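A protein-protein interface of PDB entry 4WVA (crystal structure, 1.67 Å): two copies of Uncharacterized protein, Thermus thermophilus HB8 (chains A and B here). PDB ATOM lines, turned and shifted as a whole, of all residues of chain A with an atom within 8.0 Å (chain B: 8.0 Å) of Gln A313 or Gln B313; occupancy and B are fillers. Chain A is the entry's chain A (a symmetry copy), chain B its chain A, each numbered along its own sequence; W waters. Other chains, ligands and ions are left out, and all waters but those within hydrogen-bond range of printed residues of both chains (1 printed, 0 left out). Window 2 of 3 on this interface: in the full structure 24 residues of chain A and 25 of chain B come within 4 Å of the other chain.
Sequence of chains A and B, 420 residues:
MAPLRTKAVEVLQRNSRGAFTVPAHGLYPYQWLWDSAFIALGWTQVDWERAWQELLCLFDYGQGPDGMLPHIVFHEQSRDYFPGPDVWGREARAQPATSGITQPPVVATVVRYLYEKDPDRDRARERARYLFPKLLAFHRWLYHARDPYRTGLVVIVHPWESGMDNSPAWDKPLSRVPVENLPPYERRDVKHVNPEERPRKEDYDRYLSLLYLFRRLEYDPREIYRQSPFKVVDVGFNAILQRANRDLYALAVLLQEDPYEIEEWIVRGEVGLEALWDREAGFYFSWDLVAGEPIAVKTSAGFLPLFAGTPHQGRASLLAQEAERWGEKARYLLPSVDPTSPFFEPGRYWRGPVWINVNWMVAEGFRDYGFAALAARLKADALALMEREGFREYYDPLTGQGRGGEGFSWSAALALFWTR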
ATOM      1  N   LEU A 306      22.537  39.489  10.525  1.00  0.00           N
ATOM      2  CA  LEU A 306      21.698  38.946  11.596  1.00  0.00           C
ATOM      3  C   LEU A 306      20.879  40.043  12.295  1.00  0.00           C
ATOM      4  O   LEU A 306      19.709  39.845  12.634  1.00  0.00           O
ATOM      5  CB  LEU A 306      22.558  38.212  12.614  1.00  0.00           C
ATOM      6  CG  LEU A 306      23.332  37.001  12.106  1.00  0.00           C
ATOM      7  CD1 LEU A 306      24.436  36.638  13.093  1.00  0.00           C
ATOM      8  CD2 LEU A 306      22.412  35.820  11.835  1.00  0.00           C
ATOM      9  N   THR A 310      17.540  39.584   7.849  1.00  0.00           N
ATOM     10  CA  THR A 310      17.340  39.108   6.458  1.00  0.00           C
ATOM     11  C   THR A 310      17.659  37.627   6.181  1.00  0.00           C
ATOM     12  O   THR A 310      16.998  37.012   5.336  1.00  0.00           O
ATOM     13  CB  THR A 310      18.129  39.994   5.442  1.00  0.00           C
ATOM     14  OG1 THR A 310      19.548  39.846   5.613  1.00  0.00           O
ATOM     15  CG2 THR A 310      17.751  41.436   5.568  1.00  0.00           C
ATOM     16  N   PRO A 311      18.673  37.032   6.843  1.00  0.00           N
ATOM     17  CA  PRO A 311      18.951  35.650   6.450  1.00  0.00           C
ATOM     18  C   PRO A 311      17.875  34.675   6.880  1.00  0.00           C
ATOM     19  O   PRO A 311      17.126  34.958   7.818  1.00  0.00           O
ATOM     20  CB  PRO A 311      20.228  35.292   7.225  1.00  0.00           C
ATOM     21  CG  PRO A 311      20.435  36.349   8.194  1.00  0.00           C
ATOM     22  CD  PRO A 311      19.704  37.570   7.746  1.00  0.00           C
ATOM     23  N   HIS A 312      17.811  33.532   6.212  1.00  0.00           N
ATOM     24  CA  HIS A 312      17.106  32.403   6.773  1.00  0.00           C
ATOM     25  C   HIS A 312      17.977  31.723   7.833  1.00  0.00           C
ATOM     26  O   HIS A 312      19.154  32.005   7.974  1.00  0.00           O
ATOM     27  CB  HIS A 312      16.592  31.407   5.696  1.00  0.00           C
ATOM     28  CG  HIS A 312      17.650  30.817   4.810  1.00  0.00           C
ATOM     29  ND1 HIS A 312      18.645  29.991   5.277  1.00  0.00           N
ATOM     30  CD2 HIS A 312      17.812  30.866   3.466  1.00  0.00           C
ATOM     31  CE1 HIS A 312      19.400  29.585   4.268  1.00  0.00           C
ATOM     32  NE2 HIS A 312      18.915  30.097   3.158  1.00  0.00           N
ATOM     33  N   GLN A 313      17.340  30.866   8.600  1.00  0.00           N
ATOM     34  CA  GLN A 313      17.967  30.215   9.741  1.00  0.00           C
ATOM     35  C   GLN A 313      19.191  29.390   9.388  1.00  0.00           C
ATOM     36  O   GLN A 313      20.127  29.319  10.172  1.00  0.00           O
ATOM     37  CB  GLN A 313      16.944  29.282  10.377  1.00  0.00           C
ATOM     38  CG  GLN A 313      17.365  28.665  11.691  1.00  0.00           C
ATOM     39  CD  GLN A 313      17.461  29.670  12.794  1.00  0.00           C
ATOM     40  OE1 GLN A 313      17.996  29.363  13.859  1.00  0.00           O
ATOM     41  NE2 GLN A 313      16.884  30.860  12.593  1.00  0.00           N
ATOM     42  N   GLY A 314      19.142  28.714   8.249  1.00  0.00           N
ATOM     43  CA  GLY A 314      20.282  27.922   7.773  1.00  0.00           C
ATOM     44  C   GLY A 314      21.512  28.782   7.615  1.00  0.00           C
ATOM     45  O   GLY A 314      22.605  28.440   8.080  1.00  0.00           O
ATOM     46  N   ARG A 315      21.335  29.930   6.985  1.00  0.00           N
ATOM     47  CA  ARG A 315      22.379  30.874   6.794  1.00  0.00           C
ATOM     48  C   ARG A 315      22.879  31.427   8.154  1.00  0.00           C
ATOM     49  O   ARG A 315      24.075  31.561   8.386  1.00  0.00           O
ATOM     50  CB  ARG A 315      21.868  31.988   5.900  1.00  0.00           C
ATOM     51  CG  ARG A 315      22.910  32.926   5.410  1.00  0.00           C
ATOM     52  CD  ARG A 315      22.432  33.576   4.115  1.00  0.00           C
ATOM     53  NE  ARG A 315      22.414  32.622   3.032  1.00  0.00           N
ATOM     54  CZ  ARG A 315      22.088  32.890   1.780  1.00  0.00           C
ATOM     55  NH1 ARG A 315      21.770  34.122   1.405  1.00  0.00           N
ATOM     56  NH2 ARG A 315      22.156  31.903   0.870  1.00  0.00           N
ATOM     57  N   ALA A 316      21.951  31.713   9.064  1.00  0.00           N
ATOM     58  CA  ALA A 316      22.309  32.135  10.412  1.00  0.00           C
ATOM     59  C   ALA A 316      23.120  31.046  11.130  1.00  0.00           C
ATOM     60  O   ALA A 316      24.069  31.342  11.860  1.00  0.00           O
ATOM     61  CB  ALA A 316      21.062  32.496  11.221  1.00  0.00           C
ATOM     62  N   SER A 317      22.758  29.789  10.894  1.00  0.00           N
ATOM     63  CA  SER A 317      23.485  28.680  11.506  1.00  0.00           C
ATOM     64  C   SER A 317      24.914  28.584  10.964  1.00  0.00           C
ATOM     65  O   SER A 317      25.835  28.257  11.723  1.00  0.00           O
ATOM     66  CB  SER A 317      22.713  27.352  11.367  1.00  0.00           C
ATOM     67  OG  SER A 317      23.049  26.640  10.191  1.00  0.00           O
ATOM     68  N   LEU A 318      25.116  28.883   9.682  1.00  0.00           N
ATOM     69  CA  LEU A 318      26.476  28.902   9.110  1.00  0.00           C
ATOM     70  C   LEU A 318      27.320  30.041   9.722  1.00  0.00           C
ATOM     71  O   LEU A 318      28.522  29.875  10.014  1.00  0.00           O
ATOM     72  CB  LEU A 318      26.440  28.959   7.573  1.00  0.00           C
ATOM     73  CG  LEU A 318      25.799  27.716   6.936  1.00  0.00           C
ATOM     74  CD1 LEU A 318      25.559  27.944   5.462  1.00  0.00           C
ATOM     75  CD2 LEU A 318      26.675  26.497   7.124  1.00  0.00           C
ATOM     76  N   LEU A 319      26.697  31.204   9.946  1.00  0.00           N
ATOM     77  CA  LEU A 319      27.371  32.265  10.694  1.00  0.00           C
ATOM     78  C   LEU A 319      27.691  31.846  12.140  1.00  0.00           C
ATOM     79  O   LEU A 319      28.778  32.173  12.647  1.00  0.00           O
ATOM     80  CB  LEU A 319      26.551  33.562  10.669  1.00  0.00           C
ATOM     81  CG  LEU A 319      26.501  34.315   9.341  1.00  0.00           C
ATOM     82  CD1 LEU A 319      25.606  35.555   9.459  1.00  0.00           C
ATOM     83  CD2 LEU A 319      27.905  34.729   8.903  1.00  0.00           C
ATOM     84  N   ALA A 320      26.771  31.142  12.797  1.00  0.00           N
ATOM     85  CA  ALA A 320      27.011  30.664  14.168  1.00  0.00           C
ATOM     86  C   ALA A 320      28.245  29.755  14.207  1.00  0.00           C
ATOM     87  O   ALA A 320      29.081  29.870  15.097  1.00  0.00           O
ATOM     88  CB  ALA A 320      25.801  29.945  14.717  1.00  0.00           C
ATOM     89  N   GLY A 365      21.460  39.987  17.082  1.00  0.00           N
ATOM     90  CA  GLY A 365      21.090  39.217  15.886  1.00  0.00           C
ATOM     91  C   GLY A 365      21.036  37.731  16.181  1.00  0.00           C
ATOM     92  O   GLY A 365      20.068  37.053  15.821  1.00  0.00           O
ATOM     93  N   PHE A 366      22.059  37.206  16.848  1.00  0.00           N
ATOM     94  CA  PHE A 366      22.054  35.786  17.156  1.00  0.00           C
ATOM     95  C   PHE A 366      20.882  35.403  18.052  1.00  0.00           C
ATOM     96  O   PHE A 366      20.254  34.355  17.835  1.00  0.00           O
ATOM     97  CB  PHE A 366      23.385  35.317  17.743  1.00  0.00           C
ATOM     98  CG  PHE A 366      24.428  34.977  16.711  1.00  0.00           C
ATOM     99  CD1 PHE A 366      24.168  34.018  15.721  1.00  0.00           C
ATOM    100  CD2 PHE A 366      25.679  35.567  16.738  1.00  0.00           C
ATOM    101  CE1 PHE A 366      25.116  33.695  14.784  1.00  0.00           C
ATOM    102  CE2 PHE A 366      26.643  35.228  15.807  1.00  0.00           C
ATOM    103  CZ  PHE A 366      26.366  34.287  14.830  1.00  0.00           C
ATOM    104  N   ARG A 367      20.566  36.244  19.035  1.00  0.00           N
ATOM    105  CA  ARG A 367      19.404  36.016  19.905  1.00  0.00           C
ATOM    106  C   ARG A 367      18.142  35.915  19.075  1.00  0.00           C
ATOM    107  O   ARG A 367      17.315  35.024  19.295  1.00  0.00           O
ATOM    108  CB  ARG A 367      19.277  37.135  20.947  1.00  0.00           C
ATOM    109  CG  ARG A 367      18.157  36.951  21.971  1.00  0.00           C
ATOM    110  CD  ARG A 367      16.768  37.398  21.503  1.00  0.00           C
ATOM    111  NE  ARG A 367      16.833  38.657  20.760  1.00  0.00           N
ATOM    112  CZ  ARG A 367      16.875  39.877  21.296  1.00  0.00           C
ATOM    113  NH1 ARG A 367      16.821  40.044  22.618  1.00  0.00           N
ATOM    114  NH2 ARG A 367      16.964  40.942  20.497  1.00  0.00           N
ATOM    115  N   ASP A 368      17.992  36.817  18.116  1.00  0.00           N
ATOM    116  CA  ASP A 368      16.786  36.870  17.304  1.00  0.00           C
ATOM    117  C   ASP A 368      16.625  35.582  16.480  1.00  0.00           C
ATOM    118  O   ASP A 368      15.499  35.201  16.129  1.00  0.00           O
ATOM    119  CB  ASP A 368      16.837  38.064  16.348  1.00  0.00           C
ATOM    120  CG  ASP A 368      16.733  39.409  17.047  1.00  0.00           C
ATOM    121  OD1 ASP A 368      16.287  39.482  18.220  1.00  0.00           O
ATOM    122  OD2 ASP A 368      17.078  40.429  16.389  1.00  0.00           O
ATOM    123  N   TYR A 369      17.744  34.932  16.165  1.00  0.00           N
ATOM    124  CA  TYR A 369      17.738  33.677  15.400  1.00  0.00           C
ATOM    125  C   TYR A 369      17.755  32.433  16.296  1.00  0.00           C
ATOM    126  O   TYR A 369      17.886  31.317  15.803  1.00  0.00           O
ATOM    127  CB  TYR A 369      18.894  33.668  14.369  1.00  0.00           C
ATOM    128  CG  TYR A 369      18.537  34.466  13.126  1.00  0.00           C
ATOM    129  CD1 TYR A 369      18.742  35.831  13.072  1.00  0.00           C
ATOM    130  CD2 TYR A 369      17.910  33.868  12.037  1.00  0.00           C
ATOM    131  CE1 TYR A 369      18.360  36.581  11.979  1.00  0.00           C
ATOM    132  CE2 TYR A 369      17.508  34.612  10.935  1.00  0.00           C
ATOM    133  CZ  TYR A 369      17.762  35.962  10.895  1.00  0.00           C
ATOM    134  OH  TYR A 369      17.410  36.728   9.824  1.00  0.00           O
ATOM    135  N   GLY A 370      17.605  32.606  17.606  1.00  0.00           N
ATOM    136  CA  GLY A 370      17.547  31.448  18.525  1.00  0.00           C
ATOM    137  C   GLY A 370      18.864  30.926  19.048  1.00  0.00           C
ATOM    138  O   GLY A 370      18.878  29.938  19.796  1.00  0.00           O
ATOM    139  N   PHE A 371      19.966  31.603  18.711  1.00  0.00           N
ATOM    140  CA  PHE A 371      21.308  31.190  19.120  1.00  0.00           C
ATOM    141  C   PHE A 371      21.647  31.838  20.463  1.00  0.00           C
ATOM    142  O   PHE A 371      22.495  32.724  20.574  1.00  0.00           O
ATOM    143  CB  PHE A 371      22.318  31.525  18.026  1.00  0.00           C
ATOM    144  CG  PHE A 371      22.125  30.700  16.781  1.00  0.00           C
ATOM    145  CD1 PHE A 371      21.419  31.196  15.701  1.00  0.00           C
ATOM    146  CD2 PHE A 371      22.616  29.405  16.716  1.00  0.00           C
ATOM    147  CE1 PHE A 371      21.222  30.416  14.560  1.00  0.00           C
ATOM    148  CE2 PHE A 371      22.418  28.626  15.583  1.00  0.00           C
ATOM    149  CZ  PHE A 371      21.719  29.130  14.513  1.00  0.00           C
ATOM    150  N   LEU B 306      15.065  24.666  -2.722  1.00  0.00           N
ATOM    151  CA  LEU B 306      16.235  24.846  -1.859  1.00  0.00           C
ATOM    152  C   LEU B 306      17.370  25.592  -2.578  1.00  0.00           C
ATOM    153  O   LEU B 306      18.047  26.440  -1.990  1.00  0.00           O
ATOM    154  CB  LEU B 306      16.733  23.496  -1.365  1.00  0.00           C
ATOM    155  CG  LEU B 306      15.768  22.684  -0.510  1.00  0.00           C
ATOM    156  CD1 LEU B 306      16.225  21.230  -0.446  1.00  0.00           C
ATOM    157  CD2 LEU B 306      15.610  23.283   0.880  1.00  0.00           C
ATOM    158  N   THR B 310      14.347  30.135  -1.411  1.00  0.00           N
ATOM    159  CA  THR B 310      13.047  30.721  -1.004  1.00  0.00           C
ATOM    160  C   THR B 310      12.399  30.149   0.271  1.00  0.00           C
ATOM    161  O   THR B 310      11.732  30.894   1.000  1.00  0.00           O
ATOM    162  CB  THR B 310      12.011  30.656  -2.170  1.00  0.00           C
ATOM    163  OG1 THR B 310      11.651  29.299  -2.473  1.00  0.00           O
ATOM    164  CG2 THR B 310      12.533  31.330  -3.401  1.00  0.00           C
ATOM    165  N   PRO B 311      12.543  28.838   0.557  1.00  0.00           N
ATOM    166  CA  PRO B 311      11.822  28.373   1.742  1.00  0.00           C
ATOM    167  C   PRO B 311      12.403  28.894   3.041  1.00  0.00           C
ATOM    168  O   PRO B 311      13.576  29.267   3.086  1.00  0.00           O
ATOM    169  CB  PRO B 311      12.026  26.851   1.730  1.00  0.00           C
ATOM    170  CG  PRO B 311      13.047  26.578   0.739  1.00  0.00           C
ATOM    171  CD  PRO B 311      13.121  27.725  -0.213  1.00  0.00           C
ATOM    172  N   HIS B 312      11.592  28.902   4.090  1.00  0.00           N
ATOM    173  CA  HIS B 312      12.134  29.003   5.425  1.00  0.00           C
ATOM    174  C   HIS B 312      12.679  27.642   5.868  1.00  0.00           C
ATOM    175  O   HIS B 312      12.456  26.625   5.235  1.00  0.00           O
ATOM    176  CB  HIS B 312      11.131  29.605   6.448  1.00  0.00           C
ATOM    177  CG  HIS B 312       9.840  28.856   6.598  1.00  0.00           C
ATOM    178  ND1 HIS B 312       9.767  27.576   7.095  1.00  0.00           N
ATOM    179  CD2 HIS B 312       8.557  29.247   6.398  1.00  0.00           C
ATOM    180  CE1 HIS B 312       8.502  27.192   7.159  1.00  0.00           C
ATOM    181  NE2 HIS B 312       7.747  28.187   6.745  1.00  0.00           N
ATOM    182  N   GLN B 313      13.439  27.676   6.940  1.00  0.00           N
ATOM    183  CA  GLN B 313      14.146  26.507   7.439  1.00  0.00           C
ATOM    184  C   GLN B 313      13.242  25.342   7.798  1.00  0.00           C
ATOM    185  O   GLN B 313      13.626  24.194   7.625  1.00  0.00           O
ATOM    186  CB  GLN B 313      14.905  26.912   8.697  1.00  0.00           C
ATOM    187  CG  GLN B 313      15.849  25.867   9.244  1.00  0.00           C
ATOM    188  CD  GLN B 313      17.022  25.625   8.349  1.00  0.00           C
ATOM    189  OE1 GLN B 313      17.758  24.658   8.547  1.00  0.00           O
ATOM    190  NE2 GLN B 313      17.263  26.532   7.396  1.00  0.00           N
ATOM    191  N   GLY B 314      12.083  25.645   8.366  1.00  0.00           N
ATOM    192  CA  GLY B 314      11.100  24.610   8.711  1.00  0.00           C
ATOM    193  C   GLY B 314      10.696  23.818   7.492  1.00  0.00           C
ATOM    194  O   GLY B 314      10.681  22.581   7.500  1.00  0.00           O
ATOM    195  N   ARG B 315      10.398  24.526   6.418  1.00  0.00           N
ATOM    196  CA  ARG B 315      10.043  23.933   5.176  1.00  0.00           C
ATOM    197  C   ARG B 315      11.226  23.115   4.598  1.00  0.00           C
ATOM    198  O   ARG B 315      11.052  22.006   4.105  1.00  0.00           O
ATOM    199  CB  ARG B 315       9.610  25.029   4.222  1.00  0.00           C
ATOM    200  CG  ARG B 315       8.980  24.552   2.963  1.00  0.00           C
ATOM    201  CD  ARG B 315       8.080  25.649   2.405  1.00  0.00           C
ATOM    202  NE  ARG B 315       6.908  25.828   3.229  1.00  0.00           N
ATOM    203  CZ  ARG B 315       5.921  26.672   2.986  1.00  0.00           C
ATOM    204  NH1 ARG B 315       5.922  27.429   1.897  1.00  0.00           N
ATOM    205  NH2 ARG B 315       4.872  26.698   3.827  1.00  0.00           N
ATOM    206  N   ALA B 316      12.437  23.657   4.695  1.00  0.00           N
ATOM    207  CA  ALA B 316      13.633  22.934   4.284  1.00  0.00           C
ATOM    208  C   ALA B 316      13.805  21.647   5.106  1.00  0.00           C
ATOM    209  O   ALA B 316      14.205  20.608   4.577  1.00  0.00           O
ATOM    210  CB  ALA B 316      14.876  23.818   4.406  1.00  0.00           C
ATOM    211  N   SER B 317      13.471  21.720   6.391  1.00  0.00           N
ATOM    212  CA  SER B 317      13.572  20.544   7.250  1.00  0.00           C
ATOM    213  C   SER B 317      12.562  19.467   6.841  1.00  0.00           C
ATOM    214  O   SER B 317      12.879  18.274   6.913  1.00  0.00           O
ATOM    215  CB  SER B 317      13.456  20.922   8.742  1.00  0.00           C
ATOM    216  OG  SER B 317      12.124  20.890   9.217  1.00  0.00           O
ATOM    217  N   LEU B 318      11.372  19.866   6.397  1.00  0.00           N
ATOM    218  CA  LEU B 318      10.381  18.893   5.899  1.00  0.00           C
ATOM    219  C   LEU B 318      10.870  18.218   4.599  1.00  0.00           C
ATOM    220  O   LEU B 318      10.692  17.001   4.392  1.00  0.00           O
ATOM    221  CB  LEU B 318       8.991  19.535   5.740  1.00  0.00           C
ATOM    222  CG  LEU B 318       8.390  20.012   7.070  1.00  0.00           C
ATOM    223  CD1 LEU B 318       7.161  20.857   6.821  1.00  0.00           C
ATOM    224  CD2 LEU B 318       8.027  18.840   7.955  1.00  0.00           C
ATOM    225  N   LEU B 319      11.513  18.994   3.719  1.00  0.00           N
ATOM    226  CA  LEU B 319      12.171  18.395   2.558  1.00  0.00           C
ATOM    227  C   LEU B 319      13.309  17.441   2.960  1.00  0.00           C
ATOM    228  O   LEU B 319      13.463  16.373   2.341  1.00  0.00           O
ATOM    229  CB  LEU B 319      12.679  19.476   1.594  1.00  0.00           C
ATOM    230  CG  LEU B 319      11.620  20.237   0.799  1.00  0.00           C
ATOM    231  CD1 LEU B 319      12.275  21.313  -0.076  1.00  0.00           C
ATOM    232  CD2 LEU B 319      10.813  19.280  -0.077  1.00  0.00           C
ATOM    233  N   ALA B 320      14.096  17.808   3.970  1.00  0.00           N
ATOM    234  CA  ALA B 320      15.181  16.937   4.448  1.00  0.00           C
ATOM    235  C   ALA B 320      14.618  15.590   4.914  1.00  0.00           C
ATOM    236  O   ALA B 320      15.169  14.539   4.604  1.00  0.00           O
ATOM    237  CB  ALA B 320      15.965  17.598   5.557  1.00  0.00           C
ATOM    238  N   GLY B 365      21.558  23.213  -2.348  1.00  0.00           N
ATOM    239  CA  GLY B 365      20.438  23.794  -1.594  1.00  0.00           C
ATOM    240  C   GLY B 365      20.443  23.329  -0.151  1.00  0.00           C
ATOM    241  O   GLY B 365      20.317  24.139   0.772  1.00  0.00           O
ATOM    242  N   PHE B 366      20.605  22.027   0.067  1.00  0.00           N
ATOM    243  CA  PHE B 366      20.617  21.530   1.432  1.00  0.00           C
ATOM    244  C   PHE B 366      21.771  22.114   2.238  1.00  0.00           C
ATOM    245  O   PHE B 366      21.587  22.471   3.413  1.00  0.00           O
ATOM    246  CB  PHE B 366      20.608  20.003   1.491  1.00  0.00           C
ATOM    247  CG  PHE B 366      19.234  19.391   1.399  1.00  0.00           C
ATOM    248  CD1 PHE B 366      18.231  19.745   2.313  1.00  0.00           C
ATOM    249  CD2 PHE B 366      18.941  18.436   0.443  1.00  0.00           C
ATOM    250  CE1 PHE B 366      16.981  19.185   2.243  1.00  0.00           C
ATOM    251  CE2 PHE B 366      17.688  17.855   0.383  1.00  0.00           C
ATOM    252  CZ  PHE B 366      16.705  18.224   1.286  1.00  0.00           C
ATOM    253  N   ARG B 367      22.944  22.239   1.620  1.00  0.00           N
ATOM    254  CA  ARG B 367      24.101  22.866   2.275  1.00  0.00           C
ATOM    255  C   ARG B 367      23.754  24.273   2.712  1.00  0.00           C
ATOM    256  O   ARG B 367      24.071  24.677   3.836  1.00  0.00           O
ATOM    257  CB  ARG B 367      25.317  22.875   1.338  1.00  0.00           C
ATOM    258  CG  ARG B 367      26.609  23.418   1.950  1.00  0.00           C
ATOM    259  CD  ARG B 367      26.743  24.943   1.939  1.00  0.00           C
ATOM    260  NE  ARG B 367      26.278  25.513   0.672  1.00  0.00           N
ATOM    261  CZ  ARG B 367      26.990  25.595  -0.452  1.00  0.00           C
ATOM    262  NH1 ARG B 367      28.255  25.177  -0.492  1.00  0.00           N
ATOM    263  NH2 ARG B 367      26.429  26.112  -1.547  1.00  0.00           N
ATOM    264  N   ASP B 368      23.097  25.019   1.836  1.00  0.00           N
ATOM    265  CA  ASP B 368      22.777  26.411   2.111  1.00  0.00           C
ATOM    266  C   ASP B 368      21.829  26.525   3.317  1.00  0.00           C
ATOM    267  O   ASP B 368      21.822  27.552   4.011  1.00  0.00           O
ATOM    268  CB  ASP B 368      22.108  27.057   0.895  1.00  0.00           C
ATOM    269  CG  ASP B 368      23.044  27.240  -0.287  1.00  0.00           C
ATOM    270  OD1 ASP B 368      24.290  27.198  -0.125  1.00  0.00           O
ATOM    271  OD2 ASP B 368      22.516  27.464  -1.412  1.00  0.00           O
ATOM    272  N   TYR B 369      21.029  25.486   3.548  1.00  0.00           N
ATOM    273  CA  TYR B 369      20.088  25.450   4.675  1.00  0.00           C
ATOM    274  C   TYR B 369      20.668  24.753   5.912  1.00  0.00           C
ATOM    275  O   TYR B 369      19.955  24.529   6.887  1.00  0.00           O
ATOM    276  CB  TYR B 369      18.740  24.826   4.234  1.00  0.00           C
ATOM    277  CG  TYR B 369      17.874  25.837   3.501  1.00  0.00           C
ATOM    278  CD1 TYR B 369      18.014  26.044   2.143  1.00  0.00           C
ATOM    279  CD2 TYR B 369      16.975  26.651   4.185  1.00  0.00           C
ATOM    280  CE1 TYR B 369      17.285  27.006   1.474  1.00  0.00           C
ATOM    281  CE2 TYR B 369      16.243  27.632   3.527  1.00  0.00           C
ATOM    282  CZ  TYR B 369      16.377  27.787   2.168  1.00  0.00           C
ATOM    283  OH  TYR B 369      15.660  28.717   1.477  1.00  0.00           O
ATOM    284  N   GLY B 370      21.956  24.426   5.897  1.00  0.00           N
ATOM    285  CA  GLY B 370      22.600  23.810   7.078  1.00  0.00           C
ATOM    286  C   GLY B 370      22.526  22.305   7.189  1.00  0.00           C
ATOM    287  O   GLY B 370      23.019  21.738   8.173  1.00  0.00           O
ATOM    288  N   PHE B 371      21.965  21.646   6.169  1.00  0.00           N
ATOM    289  CA  PHE B 371      21.800  20.193   6.159  1.00  0.00           C
ATOM    290  C   PHE B 371      23.041  19.548   5.541  1.00  0.00           C
ATOM    291  O   PHE B 371      23.020  18.995   4.441  1.00  0.00           O
ATOM    292  CB  PHE B 371      20.510  19.815   5.435  1.00  0.00           C
ATOM    293  CG  PHE B 371      19.274  20.245   6.182  1.00  0.00           C
ATOM    294  CD1 PHE B 371      18.621  21.419   5.858  1.00  0.00           C
ATOM    295  CD2 PHE B 371      18.798  19.489   7.241  1.00  0.00           C
ATOM    296  CE1 PHE B 371      17.491  21.824   6.571  1.00  0.00           C
ATOM    297  CE2 PHE B 371      17.676  19.893   7.954  1.00  0.00           C
ATOM    298  CZ  PHE B 371      17.031  21.059   7.621  1.00  0.00           C
HETATM  299  O   HOH W   1      23.205  29.753   3.035  1.00  0.00           O
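Of the 19 printed residues of chain B, 4 touch a printed residue of chain A. Along chain B the printed residues that touch a printed residue of chain A span positions 313 to 369. Hydrophobic or aromatic side chains of chain A that line the printed part of chain B: His A312 and Leu A318. Among the printed residues, 8 pairs touch across the chains.
N of Gly A314 sits close to NE2 of Gln B313 (3.0 Å).
Gln A313 touches just one residue of chain B: Gln B313 (3.5 Å). Printed residues of chain B within 4 Å of Leu A318: Arg B367. Gln B313 touches two residues of chain A. No residue of chain A comes within 4 Å of Gly B314. Ala B320 touches none of the printed residues of chain A. Of the printed residues of chain A, Tyr B369 touches His A312 (3.6 Å) and Gly A314 (3.5 Å). The nearest residue of chain B that does not touch Gln A313 is Tyr B369 (5.5 Å).
The backbone NH of Thr B310 sits at hydrogen-bond distance from the side-chain hydroxyl of Tyr B369 (3.5 Å). OE1 of Gln B313 sits close to O of Tyr B369 (2.8 Å). The backbone NH of Gly A314 lies close to a ring nitrogen (ND1) of His A312 (3.3 Å). A ring nitrogen (ND1) of His A312 lies within hydrogen-bond range of the backbone NH (N) of Arg A315. OE1 of Gln A313 sits close to O of Tyr A369 (2.8 Å). The backbone carbonyl oxygen of Gly A314 is in hydrogen-bond range of the side-chain hydroxyl of Ser A317 (2.8 Å).
His A312 touches Asp B368, but with the chains exchanged Asp A368 does not touch His B312 (12.0 Å). Gln B313 touches its own counterpart, Gln A313. Gly A314 touches Gln B313, but with the chains exchanged Gln A313 does not touch Gly B314 (6.4 Å). Gly A314 touches Asp B368, but with the chains exchanged Asp A368 does not touch Gly B314 (12.8 Å). Positions printed for both chains: 306, 310, 311, 312, 313, 314, 315, 316, 317, 318, 319, 320, 365, 366, 367, 368, 369, 370 and 371. Of the 8 pairs that touch across the chains among the printed residues, 1 has its exchanged pair printed and touching as well.
O of Asp B368 touches CE1 of His A312, 3.2 Å away. NE2 of His A312 touches CZ of Tyr B369, at 3.6 Å. Gln A313 touches Gln B313 (CB to CB, 3.5 Å). C of Gly A314 touches O of Asp B368, at 3.8 Å. O of Tyr B369 touches CA of Gly A314 (3.5 Å). Arg A315 touches Asp B368. Leu A318 touches Arg B367 (CD1 to O, 3.9 Å).
Water W1 bridges O of Asp B368 (2.8 Å) and NE of Arg A315 (3.0 Å).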
